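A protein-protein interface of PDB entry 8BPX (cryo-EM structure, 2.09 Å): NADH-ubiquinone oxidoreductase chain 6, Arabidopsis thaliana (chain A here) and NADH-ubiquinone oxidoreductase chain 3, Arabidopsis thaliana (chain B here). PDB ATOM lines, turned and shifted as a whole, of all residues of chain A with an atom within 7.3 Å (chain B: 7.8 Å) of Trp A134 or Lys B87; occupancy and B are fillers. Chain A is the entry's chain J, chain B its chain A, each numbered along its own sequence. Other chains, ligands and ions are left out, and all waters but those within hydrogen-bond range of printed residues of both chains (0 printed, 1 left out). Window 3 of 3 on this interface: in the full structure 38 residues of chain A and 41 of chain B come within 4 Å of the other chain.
The side-chain hydroxyl (OG) of Ser B84 sits close to the backbone carbonyl oxygen (O) of Gly A141 (3.5 Å).
The side-chain hydroxyl (OG1) of Thr A146 lies within hydrogen-bond range of the backbone carbonyl oxygen (O) of Asn A142. The backbone NH (N) of Thr A135 sits at hydrogen-bond distance from the side-chain carboxylate (OE2) of Glu A138, at 2.6 Å. The side-chain hydroxyl of Ser B84 sits at hydrogen-bond distance from the backbone carbonyl oxygen of Pro B80 (2.8 Å). The backbone carbonyl oxygen (O) of Gly B92 lies within hydrogen-bond range of the indole nitrogen (NE1) of Trp B81 (3.2 Å). OG1 of Thr A135 lies close to N of Leu A137 (3.3 Å).
Of chain B, only Lys B87 (3.7 Å) comes within 4 Å of Trp A134. Printed residues of chain B within 4 Å of Gly A141: Pro B80, Ser B84 and Ile B88. Printed residues of chain B within 4 Å of Thr A146: Ile B88 (3.7 Å), Phe B91 (3.8 Å) and Gly B92 (3.99 Å). Asn B86 touches none of the printed residues of chain A. Of the printed residues of chain A, Lys B87 touches Trp A134 and Asn A142. The nearest residue of chain B that does not touch Trp A134 is FME B1 (6.3 Å).
CE of Lys B87 touches CH2 of Trp A134 (3.7 Å). CD1 of Leu A137 touches N of Pro B80, 3.5 Å away. Val B83 touches Leu A137. Pro B80 touches Gly A141. Gly A141 touches Ile B88. OG of Ser B84 touches N of Asn A142, at 3.6 Å. Asn A142 touches Lys B87 (OD1 to CE, 3.96 Å). Thr A146 touches Ile B88 (CG2 to CB, 3.7 Å). Thr A146 touches Phe B91 (O to CE1, 3.8 Å). N of Gly B92 touches CG2 of Thr A146, 3.99 Å away.
Printed residues of chain B that touch a printed residue of chain A: Pro B80, Val B83, Ser B84, Lys B87, Ile B88, Phe B91 and Gly B92.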
ATOM      1  N   GLY A 129     -34.307 -22.585  -5.208  1.00  0.00           N
ATOM      2  CA  GLY A 129     -32.897 -22.417  -5.508  1.00  0.00           C
ATOM      3  C   GLY A 129     -32.437 -23.090  -6.785  1.00  0.00           C
ATOM      4  O   GLY A 129     -31.276 -22.914  -7.167  1.00  0.00           O
ATOM      5  N   ARG A 132     -32.385 -20.990 -11.215  1.00  0.00           N
ATOM      6  CA  ARG A 132     -31.164 -20.453 -11.825  1.00  0.00           C
ATOM      7  C   ARG A 132     -29.982 -20.876 -10.965  1.00  0.00           C
ATOM      8  O   ARG A 132     -29.579 -20.145 -10.059  1.00  0.00           O
ATOM      9  CB  ARG A 132     -31.229 -18.939 -11.959  1.00  0.00           C
ATOM     10  CG  ARG A 132     -30.004 -18.313 -12.607  1.00  0.00           C
ATOM     11  CD  ARG A 132     -30.149 -16.834 -12.780  1.00  0.00           C
ATOM     12  NE  ARG A 132     -29.003 -16.202 -13.420  1.00  0.00           N
ATOM     13  CZ  ARG A 132     -28.987 -14.948 -13.844  1.00  0.00           C
ATOM     14  NH1 ARG A 132     -30.047 -14.166 -13.719  1.00  0.00           N
ATOM     15  NH2 ARG A 132     -27.876 -14.463 -14.393  1.00  0.00           N
ATOM     16  N   SER A 133     -29.413 -22.036 -11.276  1.00  0.00           N
ATOM     17  CA  SER A 133     -28.281 -22.537 -10.516  1.00  0.00           C
ATOM     18  C   SER A 133     -26.992 -21.872 -10.982  1.00  0.00           C
ATOM     19  O   SER A 133     -26.821 -21.579 -12.167  1.00  0.00           O
ATOM     20  CB  SER A 133     -28.172 -24.057 -10.650  1.00  0.00           C
ATOM     21  OG  SER A 133     -28.348 -24.459 -11.999  1.00  0.00           O
ATOM     22  N   TRP A 134     -26.098 -21.622 -10.034  1.00  0.00           N
ATOM     23  CA  TRP A 134     -24.804 -21.014 -10.309  1.00  0.00           C
ATOM     24  C   TRP A 134     -23.727 -22.088 -10.355  1.00  0.00           C
ATOM     25  O   TRP A 134     -23.697 -22.986  -9.511  1.00  0.00           O
ATOM     26  CB  TRP A 134     -24.442 -19.980  -9.241  1.00  0.00           C
ATOM     27  CG  TRP A 134     -25.047 -18.630  -9.449  1.00  0.00           C
ATOM     28  CD1 TRP A 134     -26.132 -18.322 -10.220  1.00  0.00           C
ATOM     29  CD2 TRP A 134     -24.600 -17.394  -8.874  1.00  0.00           C
ATOM     30  NE1 TRP A 134     -26.387 -16.972 -10.162  1.00  0.00           N
ATOM     31  CE2 TRP A 134     -25.460 -16.380  -9.343  1.00  0.00           C
ATOM     32  CE3 TRP A 134     -23.553 -17.047  -8.015  1.00  0.00           C
ATOM     33  CZ2 TRP A 134     -25.309 -15.044  -8.974  1.00  0.00           C
ATOM     34  CZ3 TRP A 134     -23.404 -15.721  -7.651  1.00  0.00           C
ATOM     35  CH2 TRP A 134     -24.278 -14.737  -8.127  1.00  0.00           C
ATOM     36  N   THR A 135     -22.838 -21.986 -11.338  1.00  0.00           N
ATOM     37  CA  THR A 135     -21.652 -22.827 -11.330  1.00  0.00           C
ATOM     38  C   THR A 135     -20.697 -22.390 -10.219  1.00  0.00           C
ATOM     39  O   THR A 135     -20.761 -21.267  -9.712  1.00  0.00           O
ATOM     40  CB  THR A 135     -20.941 -22.780 -12.687  1.00  0.00           C
ATOM     41  OG1 THR A 135     -20.302 -21.510 -12.856  1.00  0.00           O
ATOM     42  CG2 THR A 135     -21.933 -23.004 -13.823  1.00  0.00           C
ATOM     43  N   ASN A 136     -19.817 -23.314  -9.828  1.00  0.00           N
ATOM     44  CA  ASN A 136     -18.722 -22.979  -8.921  1.00  0.00           C
ATOM     45  C   ASN A 136     -17.940 -21.779  -9.444  1.00  0.00           C
ATOM     46  O   ASN A 136     -17.598 -20.859  -8.685  1.00  0.00           O
ATOM     47  CB  ASN A 136     -17.819 -24.210  -8.759  1.00  0.00           C
ATOM     48  CG  ASN A 136     -16.651 -23.981  -7.814  1.00  0.00           C
ATOM     49  OD1 ASN A 136     -15.614 -24.629  -7.942  1.00  0.00           O
ATOM     50  ND2 ASN A 136     -16.817 -23.078  -6.857  1.00  0.00           N
ATOM     51  N   LEU A 137     -17.707 -21.751 -10.759  1.00  0.00           N
ATOM     52  CA  LEU A 137     -16.937 -20.684 -11.387  1.00  0.00           C
ATOM     53  C   LEU A 137     -17.589 -19.321 -11.177  1.00  0.00           C
ATOM     54  O   LEU A 137     -16.934 -18.368 -10.741  1.00  0.00           O
ATOM     55  CB  LEU A 137     -16.783 -20.990 -12.877  1.00  0.00           C
ATOM     56  CG  LEU A 137     -15.867 -20.130 -13.740  1.00  0.00           C
ATOM     57  CD1 LEU A 137     -14.477 -20.078 -13.153  1.00  0.00           C
ATOM     58  CD2 LEU A 137     -15.830 -20.662 -15.165  1.00  0.00           C
ATOM     59  N   GLU A 138     -18.883 -19.209 -11.474  1.00  0.00           N
ATOM     60  CA  GLU A 138     -19.522 -17.904 -11.368  1.00  0.00           C
ATOM     61  C   GLU A 138     -19.783 -17.497  -9.921  1.00  0.00           C
ATOM     62  O   GLU A 138     -19.741 -16.303  -9.610  1.00  0.00           O
ATOM     63  CB  GLU A 138     -20.796 -17.864 -12.214  1.00  0.00           C
ATOM     64  CG  GLU A 138     -21.885 -18.837 -11.860  1.00  0.00           C
ATOM     65  CD  GLU A 138     -22.631 -19.317 -13.102  1.00  0.00           C
ATOM     66  OE1 GLU A 138     -22.297 -18.857 -14.211  1.00  0.00           O
ATOM     67  OE2 GLU A 138     -23.545 -20.151 -12.975  1.00  0.00           O
ATOM     68  N   THR A 139     -19.989 -18.459  -9.016  1.00  0.00           N
ATOM     69  CA  THR A 139     -20.075 -18.112  -7.599  1.00  0.00           C
ATOM     70  C   THR A 139     -18.762 -17.526  -7.093  1.00  0.00           C
ATOM     71  O   THR A 139     -18.764 -16.544  -6.342  1.00  0.00           O
ATOM     72  CB  THR A 139     -20.479 -19.334  -6.769  1.00  0.00           C
ATOM     73  OG1 THR A 139     -21.598 -19.990  -7.378  1.00  0.00           O
ATOM     74  CG2 THR A 139     -20.852 -18.917  -5.348  1.00  0.00           C
ATOM     75  N   LEU A 140     -17.628 -18.111  -7.492  1.00  0.00           N
ATOM     76  CA  LEU A 140     -16.335 -17.552  -7.092  1.00  0.00           C
ATOM     77  C   LEU A 140     -16.086 -16.188  -7.737  1.00  0.00           C
ATOM     78  O   LEU A 140     -15.599 -15.252  -7.077  1.00  0.00           O
ATOM     79  CB  LEU A 140     -15.221 -18.533  -7.452  1.00  0.00           C
ATOM     80  CG  LEU A 140     -13.845 -18.304  -6.833  1.00  0.00           C
ATOM     81  CD1 LEU A 140     -13.959 -18.065  -5.338  1.00  0.00           C
ATOM     82  CD2 LEU A 140     -12.943 -19.496  -7.129  1.00  0.00           C
ATOM     83  N   GLY A 141     -16.419 -16.056  -9.024  1.00  0.00           N
ATOM     84  CA  GLY A 141     -16.170 -14.819  -9.742  1.00  0.00           C
ATOM     85  C   GLY A 141     -17.065 -13.676  -9.324  1.00  0.00           C
ATOM     86  O   GLY A 141     -16.720 -12.515  -9.566  1.00  0.00           O
ATOM     87  N   ASN A 142     -18.211 -13.979  -8.715  1.00  0.00           N
ATOM     88  CA  ASN A 142     -19.047 -12.948  -8.120  1.00  0.00           C
ATOM     89  C   ASN A 142     -18.361 -12.242  -6.952  1.00  0.00           C
ATOM     90  O   ASN A 142     -18.758 -11.129  -6.596  1.00  0.00           O
ATOM     91  CB  ASN A 142     -20.362 -13.579  -7.656  1.00  0.00           C
ATOM     92  CG  ASN A 142     -21.344 -12.565  -7.116  1.00  0.00           C
ATOM     93  OD1 ASN A 142     -21.637 -11.562  -7.762  1.00  0.00           O
ATOM     94  ND2 ASN A 142     -21.860 -12.822  -5.922  1.00  0.00           N
ATOM     95  N   LEU A 143     -17.348 -12.862  -6.351  1.00  0.00           N
ATOM     96  CA  LEU A 143     -16.732 -12.354  -5.132  1.00  0.00           C
ATOM     97  C   LEU A 143     -15.298 -11.887  -5.295  1.00  0.00           C
ATOM     98  O   LEU A 143     -14.899 -10.940  -4.615  1.00  0.00           O
ATOM     99  CB  LEU A 143     -16.753 -13.425  -4.038  1.00  0.00           C
ATOM    100  CG  LEU A 143     -18.124 -13.950  -3.633  1.00  0.00           C
ATOM    101  CD1 LEU A 143     -17.953 -15.053  -2.613  1.00  0.00           C
ATOM    102  CD2 LEU A 143     -18.971 -12.818  -3.087  1.00  0.00           C
ATOM    103  N   THR A 146     -14.817  -7.917  -6.621  1.00  0.00           N
ATOM    104  CA  THR A 146     -15.544  -6.780  -6.071  1.00  0.00           C
ATOM    105  C   THR A 146     -15.481  -6.710  -4.551  1.00  0.00           C
ATOM    106  O   THR A 146     -14.884  -5.775  -4.012  1.00  0.00           O
ATOM    107  CB  THR A 146     -16.998  -6.838  -6.556  1.00  0.00           C
ATOM    108  OG1 THR A 146     -17.531  -8.142  -6.301  1.00  0.00           O
ATOM    109  CG2 THR A 146     -17.066  -6.558  -8.046  1.00  0.00           C
ATOM    110  N   FME B   1     -24.312 -29.920 -11.505  1.00  0.00           N
ATOM    111  CN  FME B   1     -23.515 -29.139 -10.699  1.00  0.00           C
ATOM    112  O1  FME B   1     -22.685 -29.595  -9.900  1.00  0.00           O
ATOM    113  CA  FME B   1     -24.255 -31.355 -11.515  1.00  0.00           C
ATOM    114  CB  FME B   1     -25.353 -31.997 -12.390  1.00  0.00           C
ATOM    115  CG  FME B   1     -26.692 -31.341 -12.189  1.00  0.00           C
ATOM    116  SD  FME B   1     -27.248 -31.748 -10.556  1.00  0.00           S
ATOM    117  CE  FME B   1     -27.406 -33.491 -10.625  1.00  0.00           C
ATOM    118  C   FME B   1     -22.916 -31.883 -12.023  1.00  0.00           C
ATOM    119  O   FME B   1     -22.569 -31.469 -13.269  1.00  0.00           O
ATOM    120  N   PRO B  80     -12.918 -17.011 -13.908  1.00  0.00           N
ATOM    121  CA  PRO B  80     -14.122 -16.525 -13.208  1.00  0.00           C
ATOM    122  C   PRO B  80     -14.492 -15.105 -13.590  1.00  0.00           C
ATOM    123  O   PRO B  80     -15.678 -14.783 -13.697  1.00  0.00           O
ATOM    124  CB  PRO B  80     -13.740 -16.627 -11.722  1.00  0.00           C
ATOM    125  CG  PRO B  80     -12.524 -17.477 -11.676  1.00  0.00           C
ATOM    126  CD  PRO B  80     -11.811 -17.218 -12.962  1.00  0.00           C
ATOM    127  N   TRP B  81     -13.489 -14.253 -13.807  1.00  0.00           N
ATOM    128  CA  TRP B  81     -13.741 -12.877 -14.220  1.00  0.00           C
ATOM    129  C   TRP B  81     -14.495 -12.839 -15.542  1.00  0.00           C
ATOM    130  O   TRP B  81     -15.484 -12.109 -15.695  1.00  0.00           O
ATOM    131  CB  TRP B  81     -12.405 -12.138 -14.326  1.00  0.00           C
ATOM    132  CG  TRP B  81     -12.480 -10.709 -14.752  1.00  0.00           C
ATOM    133  CD1 TRP B  81     -12.848  -9.646 -13.983  1.00  0.00           C
ATOM    134  CD2 TRP B  81     -12.138 -10.178 -16.034  1.00  0.00           C
ATOM    135  NE1 TRP B  81     -12.775  -8.488 -14.711  1.00  0.00           N
ATOM    136  CE2 TRP B  81     -12.337  -8.785 -15.974  1.00  0.00           C
ATOM    137  CE3 TRP B  81     -11.689 -10.743 -17.231  1.00  0.00           C
ATOM    138  CZ2 TRP B  81     -12.103  -7.951 -17.063  1.00  0.00           C
ATOM    139  CZ3 TRP B  81     -11.456  -9.914 -18.307  1.00  0.00           C
ATOM    140  CH2 TRP B  81     -11.666  -8.533 -18.219  1.00  0.00           C
ATOM    141  N   VAL B  83     -16.403 -15.150 -16.895  1.00  0.00           N
ATOM    142  CA  VAL B  83     -17.809 -15.541 -16.798  1.00  0.00           C
ATOM    143  C   VAL B  83     -18.624 -14.598 -15.913  1.00  0.00           C
ATOM    144  O   VAL B  83     -19.858 -14.635 -15.963  1.00  0.00           O
ATOM    145  CB  VAL B  83     -17.974 -16.991 -16.310  1.00  0.00           C
ATOM    146  CG1 VAL B  83     -17.220 -17.944 -17.229  1.00  0.00           C
ATOM    147  CG2 VAL B  83     -17.520 -17.134 -14.868  1.00  0.00           C
ATOM    148  N   SER B  84     -17.980 -13.753 -15.112  1.00  0.00           N
ATOM    149  CA  SER B  84     -18.685 -12.900 -14.163  1.00  0.00           C
ATOM    150  C   SER B  84     -18.792 -11.444 -14.599  1.00  0.00           C
ATOM    151  O   SER B  84     -19.330 -10.632 -13.842  1.00  0.00           O
ATOM    152  CB  SER B  84     -17.999 -12.967 -12.795  1.00  0.00           C
ATOM    153  OG  SER B  84     -18.029 -14.283 -12.278  1.00  0.00           O
ATOM    154  N   LEU B  85     -18.289 -11.093 -15.786  1.00  0.00           N
ATOM    155  CA  LEU B  85     -18.292  -9.691 -16.206  1.00  0.00           C
ATOM    156  C   LEU B  85     -19.687  -9.071 -16.183  1.00  0.00           C
ATOM    157  O   LEU B  85     -19.822  -7.876 -15.897  1.00  0.00           O
ATOM    158  CB  LEU B  85     -17.686  -9.563 -17.601  1.00  0.00           C
ATOM    159  CG  LEU B  85     -16.187  -9.262 -17.647  1.00  0.00           C
ATOM    160  CD1 LEU B  85     -15.736  -9.020 -19.077  1.00  0.00           C
ATOM    161  CD2 LEU B  85     -15.840  -8.068 -16.764  1.00  0.00           C
ATOM    162  N   ASN B  86     -20.732  -9.851 -16.474  1.00  0.00           N
ATOM    163  CA  ASN B  86     -22.075  -9.281 -16.527  1.00  0.00           C
ATOM    164  C   ASN B  86     -22.558  -8.830 -15.153  1.00  0.00           C
ATOM    165  O   ASN B  86     -23.422  -7.951 -15.064  1.00  0.00           O
ATOM    166  CB  ASN B  86     -23.065 -10.281 -17.133  1.00  0.00           C
ATOM    167  CG  ASN B  86     -22.984 -11.662 -16.499  1.00  0.00           C
ATOM    168  OD1 ASN B  86     -22.270 -11.878 -15.521  1.00  0.00           O
ATOM    169  ND2 ASN B  86     -23.720 -12.607 -17.066  1.00  0.00           N
ATOM    170  N   LYS B  87     -22.020  -9.400 -14.080  1.00  0.00           N
ATOM    171  CA  LYS B  87     -22.465  -9.055 -12.737  1.00  0.00           C
ATOM    172  C   LYS B  87     -21.534  -8.098 -12.004  1.00  0.00           C
ATOM    173  O   LYS B  87     -22.010  -7.288 -11.205  1.00  0.00           O
ATOM    174  CB  LYS B  87     -22.645 -10.326 -11.904  1.00  0.00           C
ATOM    175  CG  LYS B  87     -23.867 -11.131 -12.304  1.00  0.00           C
ATOM    176  CD  LYS B  87     -24.138 -12.260 -11.330  1.00  0.00           C
ATOM    177  CE  LYS B  87     -22.911 -13.126 -11.164  1.00  0.00           C
ATOM    178  NZ  LYS B  87     -22.839 -14.185 -12.207  1.00  0.00           N
ATOM    179  N   ILE B  88     -20.223  -8.161 -12.249  1.00  0.00           N
ATOM    180  CA  ILE B  88     -19.301  -7.307 -11.506  1.00  0.00           C
ATOM    181  C   ILE B  88     -19.195  -5.908 -12.097  1.00  0.00           C
ATOM    182  O   ILE B  88     -18.788  -4.981 -11.387  1.00  0.00           O
ATOM    183  CB  ILE B  88     -17.902  -7.941 -11.421  1.00  0.00           C
ATOM    184  CG1 ILE B  88     -17.293  -8.099 -12.818  1.00  0.00           C
ATOM    185  CG2 ILE B  88     -17.967  -9.260 -10.679  1.00  0.00           C
ATOM    186  CD1 ILE B  88     -16.070  -8.985 -12.855  1.00  0.00           C
ATOM    187  N   ASP B  89     -19.521  -5.741 -13.373  1.00  0.00           N
ATOM    188  CA  ASP B  89     -19.670  -4.437 -14.045  1.00  0.00           C
ATOM    189  C   ASP B  89     -18.334  -3.682 -13.990  1.00  0.00           C
ATOM    190  O   ASP B  89     -17.271  -4.287 -14.191  1.00  0.00           O
ATOM    191  CB  ASP B  89     -20.839  -3.693 -13.446  1.00  0.00           C
ATOM    192  CG  ASP B  89     -21.370  -2.616 -14.369  1.00  0.00           C
ATOM    193  OD1 ASP B  89     -20.884  -2.528 -15.516  1.00  0.00           O
ATOM    194  OD2 ASP B  89     -22.272  -1.861 -13.950  1.00  0.00           O
ATOM    195  N   LEU B  90     -18.358  -2.373 -13.730  1.00  0.00           N
ATOM    196  CA  LEU B  90     -17.166  -1.549 -13.904  1.00  0.00           C
ATOM    197  C   LEU B  90     -16.133  -1.809 -12.815  1.00  0.00           C
ATOM    198  O   LEU B  90     -14.929  -1.810 -13.087  1.00  0.00           O
ATOM    199  CB  LEU B  90     -17.554  -0.072 -13.933  1.00  0.00           C
ATOM    200  CG  LEU B  90     -18.051   0.438 -15.284  1.00  0.00           C
ATOM    201  CD1 LEU B  90     -18.427   1.908 -15.201  1.00  0.00           C
ATOM    202  CD2 LEU B  90     -17.002   0.204 -16.362  1.00  0.00           C
ATOM    203  N   PHE B  91     -16.585  -2.018 -11.577  1.00  0.00           N
ATOM    204  CA  PHE B  91     -15.654  -2.230 -10.472  1.00  0.00           C
ATOM    205  C   PHE B  91     -14.799  -3.469 -10.705  1.00  0.00           C
ATOM    206  O   PHE B  91     -13.577  -3.434 -10.525  1.00  0.00           O
ATOM    207  CB  PHE B  91     -16.424  -2.343  -9.155  1.00  0.00           C
ATOM    208  CG  PHE B  91     -15.570  -2.170  -7.934  1.00  0.00           C
ATOM    209  CD1 PHE B  91     -14.722  -3.182  -7.511  1.00  0.00           C
ATOM    210  CD2 PHE B  91     -15.621  -0.996  -7.198  1.00  0.00           C
ATOM    211  CE1 PHE B  91     -13.941  -3.028  -6.389  1.00  0.00           C
ATOM    212  CE2 PHE B  91     -14.842  -0.837  -6.072  1.00  0.00           C
ATOM    213  CZ  PHE B  91     -13.999  -1.851  -5.669  1.00  0.00           C
ATOM    214  N   GLY B  92     -15.428  -4.578 -11.102  1.00  0.00           N
ATOM    215  CA  GLY B  92     -14.672  -5.793 -11.359  1.00  0.00           C
ATOM    216  C   GLY B  92     -13.718  -5.642 -12.527  1.00  0.00           C
ATOM    217  O   GLY B  92     -12.585  -6.138 -12.490  1.00  0.00           O
